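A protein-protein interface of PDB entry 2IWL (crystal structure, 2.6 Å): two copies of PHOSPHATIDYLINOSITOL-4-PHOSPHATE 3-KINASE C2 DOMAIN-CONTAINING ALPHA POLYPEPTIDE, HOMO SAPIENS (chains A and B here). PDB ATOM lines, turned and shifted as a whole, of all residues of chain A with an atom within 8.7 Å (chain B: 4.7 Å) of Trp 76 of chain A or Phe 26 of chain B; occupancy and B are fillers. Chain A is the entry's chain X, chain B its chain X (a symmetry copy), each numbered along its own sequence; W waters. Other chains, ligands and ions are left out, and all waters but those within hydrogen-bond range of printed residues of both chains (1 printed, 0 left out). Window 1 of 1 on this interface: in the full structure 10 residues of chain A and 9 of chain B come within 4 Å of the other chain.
The backbone NH (N) of Gly 80 of chain A lies within hydrogen-bond range of the side-chain hydroxyl (OG1) of Thr 27 of chain B (3.4 Å).
The backbone carbonyl oxygen (O) of Asn 112 of chain A is in hydrogen-bond range of the guanidinium group (NE) of Arg 43 of chain B (2.6 Å).
The side-chain carboxylate (OD2) of Asp 116 of chain A lies within salt-bridge range of the side-chain amino group (NZ) of Lys 77 of chain A.
The backbone carbonyl oxygen (O) of Gln 108 of chain A is in hydrogen-bond range of the side-chain amide nitrogen (ND2) of Asn 112 of chain A.
OG of Ser 114 of chain A lies within hydrogen-bond range of OD1 of Asp 116 of chain A (2.6 Å).
N of Arg 43 of chain B sits at hydrogen-bond distance from O of Ser 24 of chain B.
The backbone NH (N) of Phe 26 of chain B is in hydrogen-bond range of the backbone carbonyl oxygen (O) of Val 41 of chain B (2.7 Å).
The backbone NH (N) of Val 41 of chain B is in hydrogen-bond range of the backbone carbonyl oxygen (O) of Thr 27 of chain B (3.0 Å).
Among the printed residues, merely in contact across the chains: Leu 78 of chain A with Thr 27 of chain B, Ser 109 of chain A with Phe 26 of chain B, Trp 76 of chain A with Phe 56 of chain B, Lys 77 of chain A with Phe 26 of chain B, Trp 76 of chain A with Lys 135 of chain B, Trp 76 of chain A with Thr 27 of chain B, Pro 79 of chain A with Phe 26 of chain B, Trp 76 of chain A with His 29 of chain B, Trp 76 of chain A with Phe 26 of chain B, Ser 114 of chain A with Phe 54 of chain B, Leu 78 of chain A with Phe 26 of chain B, Ala 113 of chain A with Phe 26 of chain B and Trp 76 of chain A with Val 41 of chain B.
Of chain B, only Phe 26, Thr 27, His 29, Val 41, Phe 56 and Lys 135 come within 4 Å of Trp 76 of chain A.
Of the printed residues of chain B, Leu 78 of chain A touches Phe 26 (3.8 Å) and Thr 27 (3.5 Å).
Of the printed residues of chain B, Gly 80 of chain A touches Thr 27 (3.4 Å).
Of the printed residues of chain B, Ser 114 of chain A touches Phe 54.
Of chain A, only Trp 76 (3.8 Å), Lys 77 (3.6 Å), Leu 78 (3.8 Å), Pro 79 (3.8 Å), Ser 109 (3.6 Å) and Ala 113 (3.9 Å) come within 4 Å of Phe 26 of chain B.
Of the printed residues of chain A, Thr 27 of chain B touches Trp 76 (3.8 Å), Leu 78 (3.5 Å) and Gly 80 (3.4 Å).
Of the printed residues of chain A, His 29 of chain B touches Trp 76 (3.8 Å).
Printed residues of chain B that touch a printed residue of chain A: Phe 26, Thr 27, His 29, Val 41, Arg 43, Phe 54, Phe 56 and Lys 135.
Hydrophobic or aromatic side chains of chain B that line the printed part of chain A: Phe 26, His 29, Val 41, Phe 54 and Phe 56.
No position is printed for both chains.
Of the 15 pairs that touch across the chains among the printed residues, none has its exchanged pair printed and touching as well.
Water W1 lies within hydrogen-bond range of O of Leu 78 of chain A (2.7 Å), OG1 of Thr 27 of chain B (2.9 Å) and O of Leu 75 of chain A (3.1 Å).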
ATOM      1  N   HIS A  66     -15.784 -25.645 -22.249  1.00  0.00           N
ATOM      2  CA  HIS A  66     -15.777 -26.735 -21.297  1.00  0.00           C
ATOM      3  C   HIS A  66     -14.911 -27.832 -21.860  1.00  0.00           C
ATOM      4  O   HIS A  66     -14.102 -28.403 -21.158  1.00  0.00           O
ATOM      5  CB  HIS A  66     -17.176 -27.234 -20.996  1.00  0.00           C
ATOM      6  CG  HIS A  66     -17.201 -28.475 -20.172  1.00  0.00           C
ATOM      7  ND1 HIS A  66     -17.027 -28.458 -18.801  1.00  0.00           N
ATOM      8  CD2 HIS A  66     -17.372 -29.780 -20.526  1.00  0.00           C
ATOM      9  CE1 HIS A  66     -17.118 -29.701 -18.349  1.00  0.00           C
ATOM     10  NE2 HIS A  66     -17.314 -30.520 -19.374  1.00  0.00           N
ATOM     11  N   SER A  70     -11.342 -29.295 -20.195  1.00  0.00           N
ATOM     12  CA  SER A  70     -11.339 -30.700 -19.888  1.00  0.00           C
ATOM     13  C   SER A  70     -10.100 -31.403 -20.477  1.00  0.00           C
ATOM     14  O   SER A  70      -9.703 -32.458 -19.988  1.00  0.00           O
ATOM     15  CB  SER A  70     -12.671 -31.292 -20.325  1.00  0.00           C
ATOM     16  OG  SER A  70     -12.526 -32.087 -21.474  1.00  0.00           O
ATOM     17  N   PHE A  73      -7.743 -30.094 -17.410  1.00  0.00           N
ATOM     18  CA  PHE A  73      -8.083 -30.427 -16.034  1.00  0.00           C
ATOM     19  C   PHE A  73      -8.745 -31.758 -15.933  1.00  0.00           C
ATOM     20  O   PHE A  73      -9.539 -32.099 -16.776  1.00  0.00           O
ATOM     21  CB  PHE A  73      -9.012 -29.378 -15.466  1.00  0.00           C
ATOM     22  CG  PHE A  73      -8.342 -28.065 -15.228  1.00  0.00           C
ATOM     23  CD1 PHE A  73      -8.710 -26.946 -15.950  1.00  0.00           C
ATOM     24  CD2 PHE A  73      -7.321 -27.958 -14.286  1.00  0.00           C
ATOM     25  CE1 PHE A  73      -8.085 -25.747 -15.721  1.00  0.00           C
ATOM     26  CE2 PHE A  73      -6.685 -26.747 -14.065  1.00  0.00           C
ATOM     27  CZ  PHE A  73      -7.049 -25.650 -14.785  1.00  0.00           C
ATOM     28  N   PRO A  74      -8.451 -32.515 -14.876  1.00  0.00           N
ATOM     29  CA  PRO A  74      -9.224 -33.762 -14.740  1.00  0.00           C
ATOM     30  C   PRO A  74     -10.701 -33.387 -14.610  1.00  0.00           C
ATOM     31  O   PRO A  74     -11.019 -32.341 -14.025  1.00  0.00           O
ATOM     32  CB  PRO A  74      -8.747 -34.329 -13.408  1.00  0.00           C
ATOM     33  CG  PRO A  74      -7.514 -33.555 -13.049  1.00  0.00           C
ATOM     34  CD  PRO A  74      -7.532 -32.268 -13.751  1.00  0.00           C
ATOM     35  N   LEU A  75     -11.590 -34.223 -15.123  1.00  0.00           N
ATOM     36  CA  LEU A  75     -13.035 -33.944 -15.113  1.00  0.00           C
ATOM     37  C   LEU A  75     -13.654 -33.651 -13.757  1.00  0.00           C
ATOM     38  O   LEU A  75     -14.620 -32.887 -13.673  1.00  0.00           O
ATOM     39  CB  LEU A  75     -13.794 -35.130 -15.682  1.00  0.00           C
ATOM     40  CG  LEU A  75     -14.097 -35.129 -17.169  1.00  0.00           C
ATOM     41  CD1 LEU A  75     -14.969 -36.363 -17.483  1.00  0.00           C
ATOM     42  CD2 LEU A  75     -14.758 -33.822 -17.586  1.00  0.00           C
ATOM     43  N   TRP A  76     -13.139 -34.276 -12.705  1.00  0.00           N
ATOM     44  CA  TRP A  76     -13.722 -34.073 -11.405  1.00  0.00           C
ATOM     45  C   TRP A  76     -13.498 -32.649 -10.867  1.00  0.00           C
ATOM     46  O   TRP A  76     -14.123 -32.254  -9.883  1.00  0.00           O
ATOM     47  CB  TRP A  76     -13.229 -35.128 -10.421  1.00  0.00           C
ATOM     48  CG  TRP A  76     -11.730 -35.326 -10.368  1.00  0.00           C
ATOM     49  CD1 TRP A  76     -10.994 -36.303 -11.009  1.00  0.00           C
ATOM     50  CD2 TRP A  76     -10.789 -34.556  -9.600  1.00  0.00           C
ATOM     51  NE1 TRP A  76      -9.655 -36.163 -10.680  1.00  0.00           N
ATOM     52  CE2 TRP A  76      -9.513 -35.101  -9.826  1.00  0.00           C
ATOM     53  CE3 TRP A  76     -10.910 -33.469  -8.727  1.00  0.00           C
ATOM     54  CZ2 TRP A  76      -8.370 -34.584  -9.224  1.00  0.00           C
ATOM     55  CZ3 TRP A  76      -9.755 -32.969  -8.110  1.00  0.00           C
ATOM     56  CH2 TRP A  76      -8.517 -33.514  -8.378  1.00  0.00           C
ATOM     57  N   LYS A  77     -12.618 -31.879 -11.513  1.00  0.00           N
ATOM     58  CA  LYS A  77     -12.368 -30.505 -11.126  1.00  0.00           C
ATOM     59  C   LYS A  77     -13.349 -29.569 -11.803  1.00  0.00           C
ATOM     60  O   LYS A  77     -13.322 -28.362 -11.525  1.00  0.00           O
ATOM     61  CB  LYS A  77     -10.973 -30.065 -11.502  1.00  0.00           C
ATOM     62  CG  LYS A  77      -9.882 -30.552 -10.585  1.00  0.00           C
ATOM     63  CD  LYS A  77      -8.642 -29.698 -10.820  1.00  0.00           C
ATOM     64  CE  LYS A  77      -7.384 -30.213 -10.140  1.00  0.00           C
ATOM     65  NZ  LYS A  77      -6.719 -29.021  -9.474  1.00  0.00           N
ATOM     66  N   LEU A  78     -14.191 -30.120 -12.699  1.00  0.00           N
ATOM     67  CA  LEU A  78     -15.106 -29.300 -13.515  1.00  0.00           C
ATOM     68  C   LEU A  78     -16.568 -29.586 -13.211  1.00  0.00           C
ATOM     69  O   LEU A  78     -16.931 -30.708 -12.935  1.00  0.00           O
ATOM     70  CB  LEU A  78     -14.828 -29.513 -15.021  1.00  0.00           C
ATOM     71  CG  LEU A  78     -13.356 -29.370 -15.449  1.00  0.00           C
ATOM     72  CD1 LEU A  78     -13.209 -29.609 -16.904  1.00  0.00           C
ATOM     73  CD2 LEU A  78     -12.815 -27.997 -15.106  1.00  0.00           C
ATOM     74  N   PRO A  79     -17.418 -28.573 -13.260  1.00  0.00           N
ATOM     75  CA  PRO A  79     -18.835 -28.866 -13.118  1.00  0.00           C
ATOM     76  C   PRO A  79     -19.353 -29.626 -14.319  1.00  0.00           C
ATOM     77  O   PRO A  79     -18.764 -29.548 -15.385  1.00  0.00           O
ATOM     78  CB  PRO A  79     -19.489 -27.478 -13.071  1.00  0.00           C
ATOM     79  CG  PRO A  79     -18.498 -26.549 -13.662  1.00  0.00           C
ATOM     80  CD  PRO A  79     -17.146 -27.134 -13.415  1.00  0.00           C
ATOM     81  N   GLY A  80     -20.420 -30.397 -14.115  1.00  0.00           N
ATOM     82  CA  GLY A  80     -21.172 -31.012 -15.205  1.00  0.00           C
ATOM     83  C   GLY A  80     -21.573 -29.952 -16.219  1.00  0.00           C
ATOM     84  O   GLY A  80     -22.011 -28.822 -15.866  1.00  0.00           O
ATOM     85  N   PHE A  81     -21.331 -30.289 -17.479  1.00  0.00           N
ATOM     86  CA  PHE A  81     -21.856 -29.559 -18.614  1.00  0.00           C
ATOM     87  C   PHE A  81     -23.163 -30.244 -19.063  1.00  0.00           C
ATOM     88  O   PHE A  81     -23.256 -31.475 -19.063  1.00  0.00           O
ATOM     89  CB  PHE A  81     -20.830 -29.518 -19.742  1.00  0.00           C
ATOM     90  CG  PHE A  81     -21.078 -28.410 -20.728  1.00  0.00           C
ATOM     91  CD1 PHE A  81     -20.757 -27.073 -20.400  1.00  0.00           C
ATOM     92  CD2 PHE A  81     -21.676 -28.678 -21.963  1.00  0.00           C
ATOM     93  CE1 PHE A  81     -21.000 -26.028 -21.303  1.00  0.00           C
ATOM     94  CE2 PHE A  81     -21.926 -27.645 -22.862  1.00  0.00           C
ATOM     95  CZ  PHE A  81     -21.583 -26.311 -22.528  1.00  0.00           C
ATOM     96  N   SER A 105     -26.227 -22.387 -14.090  1.00  0.00           N
ATOM     97  CA  SER A 105     -25.692 -23.271 -13.033  1.00  0.00           C
ATOM     98  C   SER A 105     -24.255 -23.571 -13.317  1.00  0.00           C
ATOM     99  O   SER A 105     -23.415 -23.492 -12.423  1.00  0.00           O
ATOM    100  CB  SER A 105     -26.414 -24.593 -12.959  1.00  0.00           C
ATOM    101  OG  SER A 105     -27.679 -24.354 -12.433  1.00  0.00           O
ATOM    102  N   TYR A 106     -23.986 -23.883 -14.573  1.00  0.00           N
ATOM    103  CA  TYR A 106     -22.662 -24.183 -14.985  1.00  0.00           C
ATOM    104  C   TYR A 106     -21.739 -23.064 -14.588  1.00  0.00           C
ATOM    105  O   TYR A 106     -20.762 -23.350 -13.931  1.00  0.00           O
ATOM    106  CB  TYR A 106     -22.572 -24.486 -16.481  1.00  0.00           C
ATOM    107  CG  TYR A 106     -21.162 -24.860 -16.872  1.00  0.00           C
ATOM    108  CD1 TYR A 106     -20.712 -26.173 -16.716  1.00  0.00           C
ATOM    109  CD2 TYR A 106     -20.261 -23.907 -17.379  1.00  0.00           C
ATOM    110  CE1 TYR A 106     -19.410 -26.550 -17.073  1.00  0.00           C
ATOM    111  CE2 TYR A 106     -18.944 -24.278 -17.731  1.00  0.00           C
ATOM    112  CZ  TYR A 106     -18.546 -25.616 -17.568  1.00  0.00           C
ATOM    113  OH  TYR A 106     -17.297 -26.045 -17.872  1.00  0.00           O
ATOM    114  N   LEU A 107     -22.058 -21.801 -14.912  1.00  0.00           N
ATOM    115  CA  LEU A 107     -21.198 -20.650 -14.524  1.00  0.00           C
ATOM    116  C   LEU A 107     -21.024 -20.507 -13.021  1.00  0.00           C
ATOM    117  O   LEU A 107     -19.886 -20.339 -12.565  1.00  0.00           O
ATOM    118  CB  LEU A 107     -21.672 -19.313 -15.131  1.00  0.00           C
ATOM    119  CG  LEU A 107     -21.518 -19.165 -16.645  1.00  0.00           C
ATOM    120  CD1 LEU A 107     -21.839 -17.763 -17.148  1.00  0.00           C
ATOM    121  CD2 LEU A 107     -20.124 -19.642 -17.150  1.00  0.00           C
ATOM    122  N   GLN A 108     -22.122 -20.519 -12.256  1.00  0.00           N
ATOM    123  CA  GLN A 108     -22.055 -20.518 -10.782  1.00  0.00           C
ATOM    124  C   GLN A 108     -21.099 -21.582 -10.211  1.00  0.00           C
ATOM    125  O   GLN A 108     -20.282 -21.285  -9.355  1.00  0.00           O
ATOM    126  CB  GLN A 108     -23.441 -20.768 -10.186  1.00  0.00           C
ATOM    127  CG  GLN A 108     -24.198 -19.540  -9.678  1.00  0.00           C
ATOM    128  CD  GLN A 108     -24.326 -18.423 -10.672  1.00  0.00           C
ATOM    129  OE1 GLN A 108     -25.378 -17.815 -10.773  1.00  0.00           O
ATOM    130  NE2 GLN A 108     -23.268 -18.144 -11.412  1.00  0.00           N
ATOM    131  N   SER A 109     -21.204 -22.821 -10.679  1.00  0.00           N
ATOM    132  CA  SER A 109     -20.301 -23.859 -10.242  1.00  0.00           C
ATOM    133  C   SER A 109     -18.854 -23.540 -10.670  1.00  0.00           C
ATOM    134  O   SER A 109     -17.918 -23.561  -9.835  1.00  0.00           O
ATOM    135  CB  SER A 109     -20.743 -25.194 -10.807  1.00  0.00           C
ATOM    136  OG  SER A 109     -22.042 -25.474 -10.372  1.00  0.00           O
ATOM    137  N   LEU A 110     -18.665 -23.198 -11.944  1.00  0.00           N
ATOM    138  CA  LEU A 110     -17.334 -22.783 -12.357  1.00  0.00           C
ATOM    139  C   LEU A 110     -16.671 -21.807 -11.367  1.00  0.00           C
ATOM    140  O   LEU A 110     -15.517 -21.987 -11.034  1.00  0.00           O
ATOM    141  CB  LEU A 110     -17.341 -22.196 -13.773  1.00  0.00           C
ATOM    142  CG  LEU A 110     -16.024 -22.294 -14.545  1.00  0.00           C
ATOM    143  CD1 LEU A 110     -15.571 -23.789 -14.694  1.00  0.00           C
ATOM    144  CD2 LEU A 110     -16.147 -21.584 -15.927  1.00  0.00           C
ATOM    145  N   MET A 111     -17.385 -20.798 -10.874  1.00  0.00           N
ATOM    146  CA  MET A 111     -16.756 -19.845  -9.935  1.00  0.00           C
ATOM    147  C   MET A 111     -16.390 -20.470  -8.591  1.00  0.00           C
ATOM    148  O   MET A 111     -15.658 -19.875  -7.814  1.00  0.00           O
ATOM    149  CB  MET A 111     -17.660 -18.651  -9.633  1.00  0.00           C
ATOM    150  CG  MET A 111     -18.115 -17.825 -10.787  1.00  0.00           C
ATOM    151  SD  MET A 111     -16.843 -17.505 -12.009  1.00  0.00           S
ATOM    152  CE  MET A 111     -16.257 -16.008 -11.269  1.00  0.00           C
ATOM    153  N   ASN A 112     -16.936 -21.651  -8.317  1.00  0.00           N
ATOM    154  CA  ASN A 112     -16.770 -22.305  -7.019  1.00  0.00           C
ATOM    155  C   ASN A 112     -15.772 -23.477  -7.087  1.00  0.00           C
ATOM    156  O   ASN A 112     -15.584 -24.209  -6.123  1.00  0.00           O
ATOM    157  CB  ASN A 112     -18.141 -22.777  -6.508  1.00  0.00           C
ATOM    158  CG  ASN A 112     -18.964 -21.657  -5.903  1.00  0.00           C
ATOM    159  OD1 ASN A 112     -18.447 -20.858  -5.134  1.00  0.00           O
ATOM    160  ND2 ASN A 112     -20.251 -21.596  -6.243  1.00  0.00           N
ATOM    161  N   ALA A 113     -15.154 -23.619  -8.251  1.00  0.00           N
ATOM    162  CA  ALA A 113     -14.171 -24.623  -8.521  1.00  0.00           C
ATOM    163  C   ALA A 113     -12.887 -24.181  -7.881  1.00  0.00           C
ATOM    164  O   ALA A 113     -12.728 -23.003  -7.562  1.00  0.00           O
ATOM    165  CB  ALA A 113     -13.975 -24.747 -10.038  1.00  0.00           C
ATOM    166  N   SER A 114     -11.930 -25.082  -7.728  1.00  0.00           N
ATOM    167  CA  SER A 114     -10.671 -24.646  -7.148  1.00  0.00           C
ATOM    168  C   SER A 114     -10.111 -23.528  -7.977  1.00  0.00           C
ATOM    169  O   SER A 114     -10.382 -23.436  -9.165  1.00  0.00           O
ATOM    170  CB  SER A 114      -9.687 -25.801  -7.091  1.00  0.00           C
ATOM    171  OG  SER A 114      -9.558 -26.341  -8.349  1.00  0.00           O
ATOM    172  N   ASP A 116      -7.398 -22.855  -9.393  1.00  0.00           N
ATOM    173  CA  ASP A 116      -6.601 -23.081 -10.595  1.00  0.00           C
ATOM    174  C   ASP A 116      -7.488 -23.228 -11.816  1.00  0.00           C
ATOM    175  O   ASP A 116      -7.065 -22.959 -12.906  1.00  0.00           O
ATOM    176  CB  ASP A 116      -5.606 -24.241 -10.436  1.00  0.00           C
ATOM    177  CG  ASP A 116      -6.286 -25.559 -10.100  1.00  0.00           C
ATOM    178  OD1 ASP A 116      -7.490 -25.549  -9.712  1.00  0.00           O
ATOM    179  OD2 ASP A 116      -5.628 -26.626 -10.223  1.00  0.00           O
ATOM    180  N   VAL A 117      -8.739 -23.602 -11.624  1.00  0.00           N
ATOM    181  CA  VAL A 117      -9.711 -23.638 -12.703  1.00  0.00           C
ATOM    182  C   VAL A 117     -10.474 -22.290 -12.812  1.00  0.00           C
ATOM    183  O   VAL A 117     -10.529 -21.686 -13.893  1.00  0.00           O
ATOM    184  CB  VAL A 117     -10.724 -24.798 -12.470  1.00  0.00           C
ATOM    185  CG1 VAL A 117     -11.895 -24.726 -13.438  1.00  0.00           C
ATOM    186  CG2 VAL A 117     -10.016 -26.151 -12.556  1.00  0.00           C
ATOM    187  N   ALA A 118     -11.045 -21.823 -11.695  1.00  0.00           N
ATOM    188  CA  ALA A 118     -11.906 -20.633 -11.694  1.00  0.00           C
ATOM    189  C   ALA A 118     -11.189 -19.395 -12.218  1.00  0.00           C
ATOM    190  O   ALA A 118     -11.806 -18.505 -12.806  1.00  0.00           O
ATOM    191  CB  ALA A 118     -12.448 -20.367 -10.300  1.00  0.00           C
ATOM    192  N   SER B  24     -21.022 -28.417  -0.251  1.00  0.00           N
ATOM    193  CA  SER B  24     -22.035 -28.723  -1.219  1.00  0.00           C
ATOM    194  C   SER B  24     -21.543 -29.853  -2.017  1.00  0.00           C
ATOM    195  O   SER B  24     -20.360 -30.174  -1.939  1.00  0.00           O
ATOM    196  CB  SER B  24     -22.243 -27.529  -2.145  1.00  0.00           C
ATOM    197  OG  SER B  24     -21.028 -27.212  -2.774  1.00  0.00           O
ATOM    198  N   VAL B  25     -22.424 -30.442  -2.829  1.00  0.00           N
ATOM    199  CA  VAL B  25     -21.973 -31.414  -3.813  1.00  0.00           C
ATOM    200  C   VAL B  25     -21.642 -30.650  -5.093  1.00  0.00           C
ATOM    201  O   VAL B  25     -22.488 -30.010  -5.674  1.00  0.00           O
ATOM    202  CB  VAL B  25     -23.025 -32.522  -4.026  1.00  0.00           C
ATOM    203  CG1 VAL B  25     -22.508 -33.546  -4.997  1.00  0.00           C
ATOM    204  CG2 VAL B  25     -23.414 -33.200  -2.636  1.00  0.00           C
ATOM    205  N   PHE B  26     -20.398 -30.707  -5.540  1.00  0.00           N
ATOM    206  CA  PHE B  26     -19.980 -29.831  -6.609  1.00  0.00           C
ATOM    207  C   PHE B  26     -20.260 -30.433  -7.993  1.00  0.00           C
ATOM    208  O   PHE B  26     -20.685 -29.728  -8.917  1.00  0.00           O
ATOM    209  CB  PHE B  26     -18.516 -29.506  -6.394  1.00  0.00           C
ATOM    210  CG  PHE B  26     -17.826 -28.903  -7.569  1.00  0.00           C
ATOM    211  CD1 PHE B  26     -18.016 -27.545  -7.891  1.00  0.00           C
ATOM    212  CD2 PHE B  26     -16.919 -29.682  -8.338  1.00  0.00           C
ATOM    213  CE1 PHE B  26     -17.313 -26.956  -8.974  1.00  0.00           C
ATOM    214  CE2 PHE B  26     -16.218 -29.098  -9.428  1.00  0.00           C
ATOM    215  CZ  PHE B  26     -16.419 -27.731  -9.733  1.00  0.00           C
ATOM    216  N   THR B  27     -20.023 -31.729  -8.133  1.00  0.00           N
ATOM    217  CA  THR B  27     -20.276 -32.419  -9.371  1.00  0.00           C
ATOM    218  C   THR B  27     -20.297 -33.906  -9.031  1.00  0.00           C
ATOM    219  O   THR B  27     -20.151 -34.296  -7.870  1.00  0.00           O
ATOM    220  CB  THR B  27     -19.225 -32.081 -10.465  1.00  0.00           C
ATOM    221  OG1 THR B  27     -19.628 -32.654 -11.709  1.00  0.00           O
ATOM    222  CG2 THR B  27     -17.851 -32.611 -10.135  1.00  0.00           C
ATOM    223  N   HIS B  29     -18.948 -37.804 -10.590  1.00  0.00           N
ATOM    224  CA  HIS B  29     -17.865 -38.244 -11.469  1.00  0.00           C
ATOM    225  C   HIS B  29     -17.964 -39.765 -11.640  1.00  0.00           C
ATOM    226  O   HIS B  29     -18.273 -40.499 -10.664  1.00  0.00           O
ATOM    227  CB  HIS B  29     -16.531 -37.784 -10.845  1.00  0.00           C
ATOM    228  CG  HIS B  29     -15.312 -38.344 -11.497  1.00  0.00           C
ATOM    229  ND1 HIS B  29     -14.769 -37.805 -12.646  1.00  0.00           N
ATOM    230  CD2 HIS B  29     -14.512 -39.376 -11.147  1.00  0.00           C
ATOM    231  CE1 HIS B  29     -13.691 -38.494 -12.983  1.00  0.00           C
ATOM    232  NE2 HIS B  29     -13.516 -39.455 -12.091  1.00  0.00           N
ATOM    233  N   VAL B  41     -18.380 -35.507  -5.784  1.00  0.00           N
ATOM    234  CA  VAL B  41     -17.283 -34.608  -5.448  1.00  0.00           C
ATOM    235  C   VAL B  41     -17.843 -33.572  -4.533  1.00  0.00           C
ATOM    236  O   VAL B  41     -18.712 -32.767  -4.937  1.00  0.00           O
ATOM    237  CB  VAL B  41     -16.710 -33.921  -6.703  1.00  0.00           C
ATOM    238  CG1 VAL B  41     -15.536 -33.052  -6.329  1.00  0.00           C
ATOM    239  CG2 VAL B  41     -16.308 -34.996  -7.761  1.00  0.00           C
ATOM    240  N   VAL B  42     -17.364 -33.583  -3.297  1.00  0.00           N
ATOM    241  CA  VAL B  42     -17.947 -32.740  -2.283  1.00  0.00           C
ATOM    242  C   VAL B  42     -16.998 -31.599  -2.081  1.00  0.00           C
ATOM    243  O   VAL B  42     -15.767 -31.796  -1.911  1.00  0.00           O
ATOM    244  CB  VAL B  42     -18.126 -33.497  -0.976  1.00  0.00           C
ATOM    245  CG1 VAL B  42     -18.650 -32.588   0.057  1.00  0.00           C
ATOM    246  CG2 VAL B  42     -19.061 -34.790  -1.156  1.00  0.00           C
ATOM    247  N   ARG B  43     -17.552 -30.397  -2.116  1.00  0.00           N
ATOM    248  CA  ARG B  43     -16.760 -29.199  -1.995  1.00  0.00           C
ATOM    249  C   ARG B  43     -16.862 -28.696  -0.559  1.00  0.00           C
ATOM    250  O   ARG B  43     -17.984 -28.445  -0.079  1.00  0.00           O
ATOM    251  CB  ARG B  43     -17.269 -28.158  -2.966  1.00  0.00           C
ATOM    252  CG  ARG B  43     -16.456 -26.912  -2.960  1.00  0.00           C
ATOM    253  CD  ARG B  43     -17.224 -25.758  -3.652  1.00  0.00           C
ATOM    254  NE  ARG B  43     -16.410 -24.549  -3.666  1.00  0.00           N
ATOM    255  CZ  ARG B  43     -16.531 -23.529  -2.810  1.00  0.00           C
ATOM    256  NH1 ARG B  43     -17.454 -23.569  -1.868  1.00  0.00           N
ATOM    257  NH2 ARG B  43     -15.728 -22.456  -2.906  1.00  0.00           N
ATOM    258  N   PHE B  54     -11.768 -30.795  -1.658  1.00  0.00           N
ATOM    259  CA  PHE B  54     -12.696 -31.650  -2.350  1.00  0.00           C
ATOM    260  C   PHE B  54     -12.472 -33.052  -1.903  1.00  0.00           C
ATOM    261  O   PHE B  54     -11.349 -33.519  -1.879  1.00  0.00           O
ATOM    262  CB  PHE B  54     -12.454 -31.562  -3.847  1.00  0.00           C
ATOM    263  CG  PHE B  54     -12.834 -30.222  -4.431  1.00  0.00           C
ATOM    264  CD1 PHE B  54     -11.871 -29.235  -4.610  1.00  0.00           C
ATOM    265  CD2 PHE B  54     -14.175 -29.946  -4.787  1.00  0.00           C
ATOM    266  CE1 PHE B  54     -12.210 -27.992  -5.142  1.00  0.00           C
ATOM    267  CE2 PHE B  54     -14.528 -28.699  -5.317  1.00  0.00           C
ATOM    268  CZ  PHE B  54     -13.538 -27.721  -5.480  1.00  0.00           C
ATOM    269  N   PHE B  56     -14.202 -37.238  -2.081  1.00  0.00           N
ATOM    270  CA  PHE B  56     -14.939 -38.151  -2.963  1.00  0.00           C
ATOM    271  C   PHE B  56     -15.720 -39.173  -2.174  1.00  0.00           C
ATOM    272  O   PHE B  56     -15.142 -39.914  -1.376  1.00  0.00           O
ATOM    273  CB  PHE B  56     -13.967 -38.848  -3.929  1.00  0.00           C
ATOM    274  CG  PHE B  56     -13.208 -37.882  -4.795  1.00  0.00           C
ATOM    275  CD1 PHE B  56     -11.891 -37.556  -4.505  1.00  0.00           C
ATOM    276  CD2 PHE B  56     -13.828 -37.273  -5.891  1.00  0.00           C
ATOM    277  CE1 PHE B  56     -11.183 -36.638  -5.304  1.00  0.00           C
ATOM    278  CE2 PHE B  56     -13.136 -36.356  -6.692  1.00  0.00           C
ATOM    279  CZ  PHE B  56     -11.803 -36.040  -6.394  1.00  0.00           C
ATOM    280  N   LYS B 100     -27.225 -35.883  -6.944  1.00  0.00           N
ATOM    281  CA  LYS B 100     -26.367 -34.715  -6.716  1.00  0.00           C
ATOM    282  C   LYS B 100     -27.143 -33.607  -6.061  1.00  0.00           C
ATOM    283  O   LYS B 100     -26.704 -33.090  -5.037  1.00  0.00           O
ATOM    284  CB  LYS B 100     -25.730 -34.194  -8.014  1.00  0.00           C
ATOM    285  CG  LYS B 100     -24.975 -32.838  -7.906  1.00  0.00           C
ATOM    286  CD  LYS B 100     -24.922 -32.151  -9.272  1.00  0.00           C
ATOM    287  CE  LYS B 100     -24.308 -30.755  -9.232  1.00  0.00           C
ATOM    288  NZ  LYS B 100     -25.224 -29.702  -8.701  1.00  0.00           N
ATOM    289  N   LYS B 135      -5.609 -35.787  -3.892  1.00  0.00           N
ATOM    290  CA  LYS B 135      -5.938 -35.462  -5.297  1.00  0.00           C
ATOM    291  C   LYS B 135      -5.592 -36.490  -6.385  1.00  0.00           C
ATOM    292  O   LYS B 135      -6.498 -37.044  -7.033  1.00  0.00           O
ATOM    293  CB  LYS B 135      -5.426 -34.050  -5.652  1.00  0.00           C
ATOM    294  CG  LYS B 135      -6.421 -32.887  -5.377  1.00  0.00           C
ATOM    295  CD  LYS B 135      -7.032 -32.806  -3.945  1.00  0.00           C
ATOM    296  CE  LYS B 135      -7.733 -31.445  -3.727  1.00  0.00           C
ATOM    297  NZ  LYS B 135      -8.619 -31.304  -2.488  1.00  0.00           N
HETATM  298  O   HOH W   1     -17.706 -33.096 -13.839  1.00  0.00           O
